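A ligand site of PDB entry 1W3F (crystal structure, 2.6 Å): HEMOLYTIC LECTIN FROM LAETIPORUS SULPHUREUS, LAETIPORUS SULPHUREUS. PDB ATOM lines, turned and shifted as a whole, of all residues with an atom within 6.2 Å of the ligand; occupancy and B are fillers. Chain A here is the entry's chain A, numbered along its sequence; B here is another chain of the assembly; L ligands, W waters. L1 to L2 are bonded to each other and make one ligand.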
ATOM      1  N   ARG A  76      24.270 -14.747  11.521  1.00  0.00           N
ATOM      2  CA  ARG A  76      23.480 -15.525  10.584  1.00  0.00           C
ATOM      3  C   ARG A  76      22.328 -16.287  11.205  1.00  0.00           C
ATOM      4  O   ARG A  76      21.248 -16.407  10.610  1.00  0.00           O
ATOM      5  CB  ARG A  76      24.366 -16.488   9.780  1.00  0.00           C
ATOM      6  CG  ARG A  76      24.690 -15.936   8.420  1.00  0.00           C
ATOM      7  CD  ARG A  76      23.417 -15.629   7.658  1.00  0.00           C
ATOM      8  NE  ARG A  76      23.620 -14.632   6.621  1.00  0.00           N
ATOM      9  CZ  ARG A  76      22.783 -14.436   5.604  1.00  0.00           C
ATOM     10  NH1 ARG A  76      21.694 -15.172   5.502  1.00  0.00           N
ATOM     11  NH2 ARG A  76      23.037 -13.503   4.702  1.00  0.00           N
ATOM     12  N   GLU A  79      17.473 -13.468  13.600  1.00  0.00           N
ATOM     13  CA  GLU A  79      16.989 -12.388  12.756  1.00  0.00           C
ATOM     14  C   GLU A  79      16.653 -11.182  13.630  1.00  0.00           C
ATOM     15  O   GLU A  79      16.145 -11.336  14.743  1.00  0.00           O
ATOM     16  CB  GLU A  79      15.743 -12.846  12.003  1.00  0.00           C
ATOM     17  CG  GLU A  79      15.546 -12.196  10.648  1.00  0.00           C
ATOM     18  CD  GLU A  79      16.483 -12.751   9.591  1.00  0.00           C
ATOM     19  OE1 GLU A  79      16.339 -13.945   9.220  1.00  0.00           O
ATOM     20  OE2 GLU A  79      17.365 -12.006   9.126  1.00  0.00           O
ATOM     21  N   TYR A  81      19.638 -10.193  10.759  1.00  0.00           N
ATOM     22  CA  TYR A  81      21.070 -10.462  10.694  1.00  0.00           C
ATOM     23  C   TYR A  81      21.983  -9.284  11.043  1.00  0.00           C
ATOM     24  O   TYR A  81      23.140  -9.493  11.392  1.00  0.00           O
ATOM     25  CB  TYR A  81      21.442 -11.033   9.329  1.00  0.00           C
ATOM     26  CG  TYR A  81      20.675 -12.282   8.963  1.00  0.00           C
ATOM     27  CD1 TYR A  81      20.116 -13.103   9.939  1.00  0.00           C
ATOM     28  CD2 TYR A  81      20.524 -12.658   7.624  1.00  0.00           C
ATOM     29  CE1 TYR A  81      19.414 -14.260   9.595  1.00  0.00           C
ATOM     30  CE2 TYR A  81      19.831 -13.810   7.278  1.00  0.00           C
ATOM     31  CZ  TYR A  81      19.282 -14.598   8.266  1.00  0.00           C
ATOM     32  OH  TYR A  81      18.580 -15.730   7.915  1.00  0.00           O
ATOM     33  N   LEU A 120      29.225  -7.579   5.717  1.00  0.00           N
ATOM     34  CA  LEU A 120      28.204  -6.544   5.595  1.00  0.00           C
ATOM     35  C   LEU A 120      27.869  -6.248   4.141  1.00  0.00           C
ATOM     36  O   LEU A 120      28.740  -6.284   3.268  1.00  0.00           O
ATOM     37  CB  LEU A 120      28.620  -5.263   6.319  1.00  0.00           C
ATOM     38  CG  LEU A 120      28.527  -5.336   7.845  1.00  0.00           C
ATOM     39  CD1 LEU A 120      28.874  -3.998   8.436  1.00  0.00           C
ATOM     40  CD2 LEU A 120      27.129  -5.773   8.261  1.00  0.00           C
ATOM     41  N   VAL A 121      26.600  -5.945   3.918  1.00  0.00           N
ATOM     42  CA  VAL A 121      26.079  -5.645   2.591  1.00  0.00           C
ATOM     43  C   VAL A 121      25.432  -4.260   2.533  1.00  0.00           C
ATOM     44  O   VAL A 121      24.709  -3.858   3.467  1.00  0.00           O
ATOM     45  CB  VAL A 121      25.023  -6.716   2.173  1.00  0.00           C
ATOM     46  CG1 VAL A 121      24.360  -6.328   0.862  1.00  0.00           C
ATOM     47  CG2 VAL A 121      25.675  -8.081   2.064  1.00  0.00           C
ATOM     48  N   ARG A 123      23.461  -2.224  -0.525  1.00  0.00           N
ATOM     49  CA  ARG A 123      22.944  -2.171  -1.899  1.00  0.00           C
ATOM     50  C   ARG A 123      21.585  -1.477  -1.990  1.00  0.00           C
ATOM     51  O   ARG A 123      20.893  -1.309  -0.986  1.00  0.00           O
ATOM     52  CB  ARG A 123      22.761  -3.601  -2.403  1.00  0.00           C
ATOM     53  CG  ARG A 123      21.694  -4.331  -1.603  1.00  0.00           C
ATOM     54  CD  ARG A 123      21.790  -5.833  -1.703  1.00  0.00           C
ATOM     55  NE  ARG A 123      20.931  -6.439  -0.692  1.00  0.00           N
ATOM     56  CZ  ARG A 123      20.795  -7.744  -0.495  1.00  0.00           C
ATOM     57  NH1 ARG A 123      21.451  -8.625  -1.237  1.00  0.00           N
ATOM     58  NH2 ARG A 123      19.976  -8.172   0.470  1.00  0.00           N
ATOM     59  N   HIS A 125      19.663  -2.264  -4.974  1.00  0.00           N
ATOM     60  CA  HIS A 125      18.997  -3.064  -6.006  1.00  0.00           C
ATOM     61  C   HIS A 125      18.166  -4.214  -5.436  1.00  0.00           C
ATOM     62  O   HIS A 125      17.340  -4.798  -6.147  1.00  0.00           O
ATOM     63  CB  HIS A 125      20.049  -3.624  -6.982  1.00  0.00           C
ATOM     64  CG  HIS A 125      20.885  -4.726  -6.409  1.00  0.00           C
ATOM     65  ND1 HIS A 125      20.658  -6.056  -6.699  1.00  0.00           N
ATOM     66  CD2 HIS A 125      21.942  -4.705  -5.564  1.00  0.00           C
ATOM     67  CE1 HIS A 125      21.530  -6.805  -6.045  1.00  0.00           C
ATOM     68  NE2 HIS A 125      22.322  -6.005  -5.345  1.00  0.00           N
ATOM     69  N   LEU A 126      18.371  -4.544  -4.166  1.00  0.00           N
ATOM     70  CA  LEU A 126      17.668  -5.662  -3.548  1.00  0.00           C
ATOM     71  C   LEU A 126      17.535  -5.430  -2.048  1.00  0.00           C
ATOM     72  O   LEU A 126      18.411  -4.844  -1.424  1.00  0.00           O
ATOM     73  CB  LEU A 126      18.449  -6.944  -3.846  1.00  0.00           C
ATOM     74  CG  LEU A 126      18.012  -8.349  -3.421  1.00  0.00           C
ATOM     75  CD1 LEU A 126      18.205  -8.497  -1.937  1.00  0.00           C
ATOM     76  CD2 LEU A 126      16.575  -8.605  -3.821  1.00  0.00           C
ATOM     77  N   GLN A 127      16.420  -5.870  -1.468  1.00  0.00           N
ATOM     78  CA  GLN A 127      16.185  -5.706  -0.020  1.00  0.00           C
ATOM     79  C   GLN A 127      16.490  -6.968   0.765  1.00  0.00           C
ATOM     80  O   GLN A 127      16.334  -8.083   0.266  1.00  0.00           O
ATOM     81  CB  GLN A 127      14.736  -5.303   0.247  1.00  0.00           C
ATOM     82  CG  GLN A 127      14.386  -3.889  -0.152  1.00  0.00           C
ATOM     83  CD  GLN A 127      12.964  -3.541   0.197  1.00  0.00           C
ATOM     84  OE1 GLN A 127      12.511  -2.407  -0.007  1.00  0.00           O
ATOM     85  NE2 GLN A 127      12.225  -4.500   0.733  1.00  0.00           N
ATOM     86  N   PRO A 128      16.933  -6.808   2.027  1.00  0.00           N
ATOM     87  CA  PRO A 128      17.143  -5.505   2.693  1.00  0.00           C
ATOM     88  C   PRO A 128      18.357  -4.797   2.105  1.00  0.00           C
ATOM     89  O   PRO A 128      19.338  -5.431   1.703  1.00  0.00           O
ATOM     90  CB  PRO A 128      17.364  -5.893   4.154  1.00  0.00           C
ATOM     91  CG  PRO A 128      16.691  -7.230   4.283  1.00  0.00           C
ATOM     92  CD  PRO A 128      17.075  -7.907   2.989  1.00  0.00           C
ATOM     93  N   TRP A 131      22.279  -5.279   4.853  1.00  0.00           N
ATOM     94  CA  TRP A 131      22.156  -6.654   5.321  1.00  0.00           C
ATOM     95  C   TRP A 131      23.549  -7.271   5.348  1.00  0.00           C
ATOM     96  O   TRP A 131      24.533  -6.552   5.433  1.00  0.00           O
ATOM     97  CB  TRP A 131      21.281  -7.416   4.312  1.00  0.00           C
ATOM     98  CG  TRP A 131      20.482  -8.538   4.876  1.00  0.00           C
ATOM     99  CD1 TRP A 131      20.384  -9.804   4.361  1.00  0.00           C
ATOM    100  CD2 TRP A 131      19.611  -8.493   6.001  1.00  0.00           C
ATOM    101  NE1 TRP A 131      19.511 -10.547   5.112  1.00  0.00           N
ATOM    102  CE2 TRP A 131      19.009  -9.764   6.123  1.00  0.00           C
ATOM    103  CE3 TRP A 131      19.272  -7.497   6.929  1.00  0.00           C
ATOM    104  CZ2 TRP A 131      18.098 -10.079   7.131  1.00  0.00           C
ATOM    105  CZ3 TRP A 131      18.355  -7.799   7.938  1.00  0.00           C
ATOM    106  CH2 TRP A 131      17.781  -9.073   8.026  1.00  0.00           C
ATOM    107  N   ASN A 132      23.623  -8.602   5.321  1.00  0.00           N
ATOM    108  CA  ASN A 132      24.919  -9.260   5.272  1.00  0.00           C
ATOM    109  C   ASN A 132      24.850 -10.479   4.364  1.00  0.00           C
ATOM    110  O   ASN A 132      23.788 -10.818   3.863  1.00  0.00           O
ATOM    111  CB  ASN A 132      25.467  -9.652   6.661  1.00  0.00           C
ATOM    112  CG  ASN A 132      24.688 -10.772   7.336  1.00  0.00           C
ATOM    113  OD1 ASN A 132      24.123 -11.652   6.683  1.00  0.00           O
ATOM    114  ND2 ASN A 132      24.696 -10.749   8.670  1.00  0.00           N
ATOM    115  N   HIS A 133      25.986 -11.122   4.135  1.00  0.00           N
ATOM    116  CA  HIS A 133      26.067 -12.252   3.227  1.00  0.00           C
ATOM    117  C   HIS A 133      27.175 -13.210   3.691  1.00  0.00           C
ATOM    118  O   HIS A 133      28.082 -12.815   4.428  1.00  0.00           O
ATOM    119  CB  HIS A 133      26.379 -11.718   1.826  1.00  0.00           C
ATOM    120  CG  HIS A 133      26.119 -12.690   0.725  1.00  0.00           C
ATOM    121  ND1 HIS A 133      24.847 -13.089   0.377  1.00  0.00           N
ATOM    122  CD2 HIS A 133      26.965 -13.330  -0.120  1.00  0.00           C
ATOM    123  CE1 HIS A 133      24.917 -13.943  -0.634  1.00  0.00           C
ATOM    124  NE2 HIS A 133      26.191 -14.100  -0.953  1.00  0.00           N
ATOM    125  N   GLU A 137      31.227 -15.777  -0.353  1.00  0.00           N
ATOM    126  CA  GLU A 137      30.768 -15.318  -1.651  1.00  0.00           C
ATOM    127  C   GLU A 137      30.928 -13.790  -1.705  1.00  0.00           C
ATOM    128  O   GLU A 137      30.141 -13.059  -1.109  1.00  0.00           O
ATOM    129  CB  GLU A 137      29.295 -15.673  -1.870  1.00  0.00           C
ATOM    130  CG  GLU A 137      29.054 -16.691  -2.967  1.00  0.00           C
ATOM    131  CD  GLU A 137      27.748 -16.451  -3.700  1.00  0.00           C
ATOM    132  OE1 GLU A 137      26.705 -16.327  -3.034  1.00  0.00           O
ATOM    133  OE2 GLU A 137      27.760 -16.378  -4.953  1.00  0.00           O
ATOM    134  N   VAL A 138      31.931 -13.325  -2.424  1.00  0.00           N
ATOM    135  CA  VAL A 138      32.203 -11.904  -2.525  1.00  0.00           C
ATOM    136  C   VAL A 138      31.528 -11.178  -3.695  1.00  0.00           C
ATOM    137  O   VAL A 138      31.712 -11.545  -4.857  1.00  0.00           O
ATOM    138  CB  VAL A 138      33.731 -11.646  -2.630  1.00  0.00           C
ATOM    139  CG1 VAL A 138      34.023 -10.175  -2.513  1.00  0.00           C
ATOM    140  CG2 VAL A 138      34.465 -12.420  -1.541  1.00  0.00           C
ATOM    141  N   PHE A 139      30.749 -10.156  -3.364  1.00  0.00           N
ATOM    142  CA  PHE A 139      30.061  -9.316  -4.354  1.00  0.00           C
ATOM    143  C   PHE A 139      30.480  -7.879  -4.101  1.00  0.00           C
ATOM    144  O   PHE A 139      30.811  -7.504  -2.974  1.00  0.00           O
ATOM    145  CB  PHE A 139      28.541  -9.420  -4.224  1.00  0.00           C
ATOM    146  CG  PHE A 139      27.955 -10.687  -4.773  1.00  0.00           C
ATOM    147  CD1 PHE A 139      27.718 -11.777  -3.944  1.00  0.00           C
ATOM    148  CD2 PHE A 139      27.596 -10.764  -6.109  1.00  0.00           C
ATOM    149  CE1 PHE A 139      27.116 -12.930  -4.450  1.00  0.00           C
ATOM    150  CE2 PHE A 139      27.001 -11.914  -6.630  1.00  0.00           C
ATOM    151  CZ  PHE A 139      26.764 -13.004  -5.801  1.00  0.00           C
ATOM    152  N   ASP A 140      30.455  -7.049  -5.137  1.00  0.00           N
ATOM    153  CA  ASP A 140      30.843  -5.647  -5.007  1.00  0.00           C
ATOM    154  C   ASP A 140      30.063  -4.845  -3.983  1.00  0.00           C
ATOM    155  O   ASP A 140      30.580  -3.872  -3.438  1.00  0.00           O
ATOM    156  CB  ASP A 140      30.738  -4.930  -6.365  1.00  0.00           C
ATOM    157  CG  ASP A 140      31.959  -5.125  -7.234  1.00  0.00           C
ATOM    158  OD1 ASP A 140      32.999  -5.595  -6.723  1.00  0.00           O
ATOM    159  OD2 ASP A 140      31.894  -4.788  -8.442  1.00  0.00           O
ATOM    160  N   ASP A 141      28.818  -5.237  -3.703  1.00  0.00           N
ATOM    161  CA  ASP A 141      28.015  -4.494  -2.753  1.00  0.00           C
ATOM    162  C   ASP A 141      28.389  -4.729  -1.307  1.00  0.00           C
ATOM    163  O   ASP A 141      27.678  -4.312  -0.397  1.00  0.00           O
ATOM    164  CB  ASP A 141      26.508  -4.758  -2.953  1.00  0.00           C
ATOM    165  CG  ASP A 141      26.145  -6.240  -2.950  1.00  0.00           C
ATOM    166  OD1 ASP A 141      26.911  -7.071  -2.405  1.00  0.00           O
ATOM    167  OD2 ASP A 141      25.071  -6.566  -3.492  1.00  0.00           O
ATOM    168  N   GLN A 142      29.509  -5.402  -1.102  1.00  0.00           N
ATOM    169  CA  GLN A 142      30.016  -5.692   0.228  1.00  0.00           C
ATOM    170  C   GLN A 142      31.138  -4.713   0.564  1.00  0.00           C
ATOM    171  O   GLN A 142      31.719  -4.756   1.654  1.00  0.00           O
ATOM    172  CB  GLN A 142      30.561  -7.124   0.283  1.00  0.00           C
ATOM    173  CG  GLN A 142      29.499  -8.189   0.556  1.00  0.00           C
ATOM    174  CD  GLN A 142      29.916  -9.575   0.080  1.00  0.00           C
ATOM    175  OE1 GLN A 142      31.057  -9.987   0.257  1.00  0.00           O
ATOM    176  NE2 GLN A 142      28.992 -10.295  -0.511  1.00  0.00           N
ATOM    177  N   SER B  37      23.836  -8.601 -12.455  1.00  0.00           N
ATOM    178  CA  SER B  37      24.317  -8.910 -11.128  1.00  0.00           C
ATOM    179  C   SER B  37      25.544  -8.128 -10.714  1.00  0.00           C
ATOM    180  O   SER B  37      26.373  -7.749 -11.551  1.00  0.00           O
ATOM    181  CB  SER B  37      24.666 -10.399 -11.015  1.00  0.00           C
ATOM    182  OG  SER B  37      25.446 -10.626  -9.843  1.00  0.00           O
ATOM    183  N   PRO B  38      25.664  -7.854  -9.411  1.00  0.00           N
ATOM    184  CA  PRO B  38      26.817  -7.115  -8.904  1.00  0.00           C
ATOM    185  C   PRO B  38      27.994  -8.051  -9.199  1.00  0.00           C
ATOM    186  O   PRO B  38      27.804  -9.270  -9.282  1.00  0.00           O
ATOM    187  CB  PRO B  38      26.540  -7.016  -7.405  1.00  0.00           C
ATOM    188  CG  PRO B  38      25.043  -7.017  -7.338  1.00  0.00           C
ATOM    189  CD  PRO B  38      24.668  -8.069  -8.345  1.00  0.00           C
HETATM  190  C1  LIG L   1      18.643 -14.274   0.278  1.00  0.00           C
HETATM  191  C2  LIG L   1      19.238 -12.910   0.796  1.00  0.00           C
HETATM  192  C3  LIG L   1      19.711 -12.132  -0.444  1.00  0.00           C
HETATM  193  C4  LIG L   1      20.775 -12.926  -1.218  1.00  0.00           C
HETATM  194  C5  LIG L   1      20.220 -14.364  -1.619  1.00  0.00           C
HETATM  195  C6  LIG L   1      21.244 -15.433  -1.971  1.00  0.00           C
HETATM  196  C7  LIG L   1      17.999 -12.345   2.840  1.00  0.00           C
HETATM  197  C8  LIG L   1      16.895 -11.480   3.433  1.00  0.00           C
HETATM  198  O1  LIG L   1      19.658 -14.953  -0.445  1.00  0.00           O
HETATM  199  O2  LIG L   1      20.266 -10.875  -0.083  1.00  0.00           O
HETATM  200  O3  LIG L   1      21.121 -12.142  -2.363  1.00  0.00           O
HETATM  201  O4  LIG L   1      21.911 -15.112  -3.044  1.00  0.00           O
HETATM  202  O5  LIG L   1      18.642 -13.179   3.544  1.00  0.00           O
HETATM  203  N1  LIG L   1      18.224 -12.154   1.518  1.00  0.00           N
HETATM  204  O6  LIG L   1      17.538 -14.087  -0.547  1.00  0.00           O
HETATM  205  C1  LG2 L   2      22.351 -11.678  -2.684  1.00  0.00           C
HETATM  206  C2  LG2 L   2      22.253 -11.075  -4.142  1.00  0.00           C
HETATM  207  C3  LG2 L   2      23.596 -10.464  -4.658  1.00  0.00           C
HETATM  208  C4  LG2 L   2      24.311  -9.647  -3.564  1.00  0.00           C
HETATM  209  C5  LG2 L   2      24.440 -10.474  -2.252  1.00  0.00           C
HETATM  210  C6  LG2 L   2      25.161  -9.694  -1.151  1.00  0.00           C
HETATM  211  O1  LG2 L   2      21.829 -12.042  -5.113  1.00  0.00           O
HETATM  212  O2  LG2 L   2      23.331  -9.624  -5.789  1.00  0.00           O
HETATM  213  O3  LG2 L   2      23.565  -8.471  -3.314  1.00  0.00           O
HETATM  214  O4  LG2 L   2      23.147 -10.879  -1.791  1.00  0.00           O
HETATM  215  O5  LG2 L   2      26.539  -9.656  -1.369  1.00  0.00           O
HETATM  216  O   HOH W   1      16.257 -10.747  -0.294  1.00  0.00           O
HETATM  217  O   HOH W   2      19.080 -12.427  -5.786  1.00  0.00           O
HETATM  218  O   HOH W   3      22.777 -12.028   1.556  1.00  0.00           O
HETATM  219  O   HOH W   4      23.386 -11.476  -7.873  1.00  0.00           O
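An oxygen (O3) of LG2 L2 sits at hydrogen-bond distance from the side-chain carboxylate of Asp 141, 2.4 Å away.
An oxygen (O5) of LG2 L2 is in hydrogen-bond range of the side-chain amide nitrogen (NE2) of Gln 142.
The guanidinium group of Arg 123 lies within hydrogen-bond range of an oxygen (O2) of LIG L1, 2.8 Å away.
NE1 of Trp 131 lies within hydrogen-bond range of O5 of LIG L1 (3.2 Å).
A ring nitrogen (NE2) of His 125 lies within hydrogen-bond range of an oxygen (O3) of LG2 L2 (3.4 Å).
Water W4 lies within hydrogen-bond range of an oxygen (O2) of LG2 L2 and the side-chain hydroxyl of Ser 37 of chain B.
Water W1 bridges O of Gln 127 (2.7 Å) and N1 of LIG L1 (3.0 Å).
Water W3 lies within hydrogen-bond range of a ring nitrogen (ND1) of His 133 (2.6 Å), the backbone carbonyl oxygen (O) of Asn 132 (2.8 Å), an oxygen (O2) of LIG L1 (3.2 Å) and the guanidinium group (NH2) of Arg 76 (3.5 Å).
Residues that only touch the ligand: Tyr 81, Val 121, Leu 126, Pro 128, His 133, Phe 139 and Pro 38 of chain B.
12 residues have an atom within 4 Å of the ligand: Tyr 81, Val 121, Arg 123, His 125, Leu 126, Pro 128, Trp 131, His 133, Phe 139, Asp 141, Gln 142 and Pro 38 of chain B.
OD2 of Asp 141 lies within hydrogen-bond range of NE2 of His 125.
The side-chain amide nitrogen (NE2) of Gln 142 sits close to the backbone NH (N) of Phe 139, 3.4 Å away.
The backbone carbonyl oxygen of Pro 128 lies within hydrogen-bond range of the guanidinium group of Arg 123, at 3.0 Å.
NE of Arg 123 is in hydrogen-bond range of O of Leu 126 (3.1 Å).
The backbone carbonyl oxygen (O) of Trp 131 lies within hydrogen-bond range of the backbone NH (N) of Val 121, 2.6 Å away.
NE2 of His 133 lies within hydrogen-bond range of OE1 of Glu 137 (3.1 Å).
The backbone carbonyl oxygen (O) of Tyr 81 lies close to the side-chain amide nitrogen (ND2) of Asn 132, at 3.4 Å.
The side-chain hydroxyl of Tyr 81 sits close to the side-chain carboxylate of Glu 79, at 3.1 Å.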
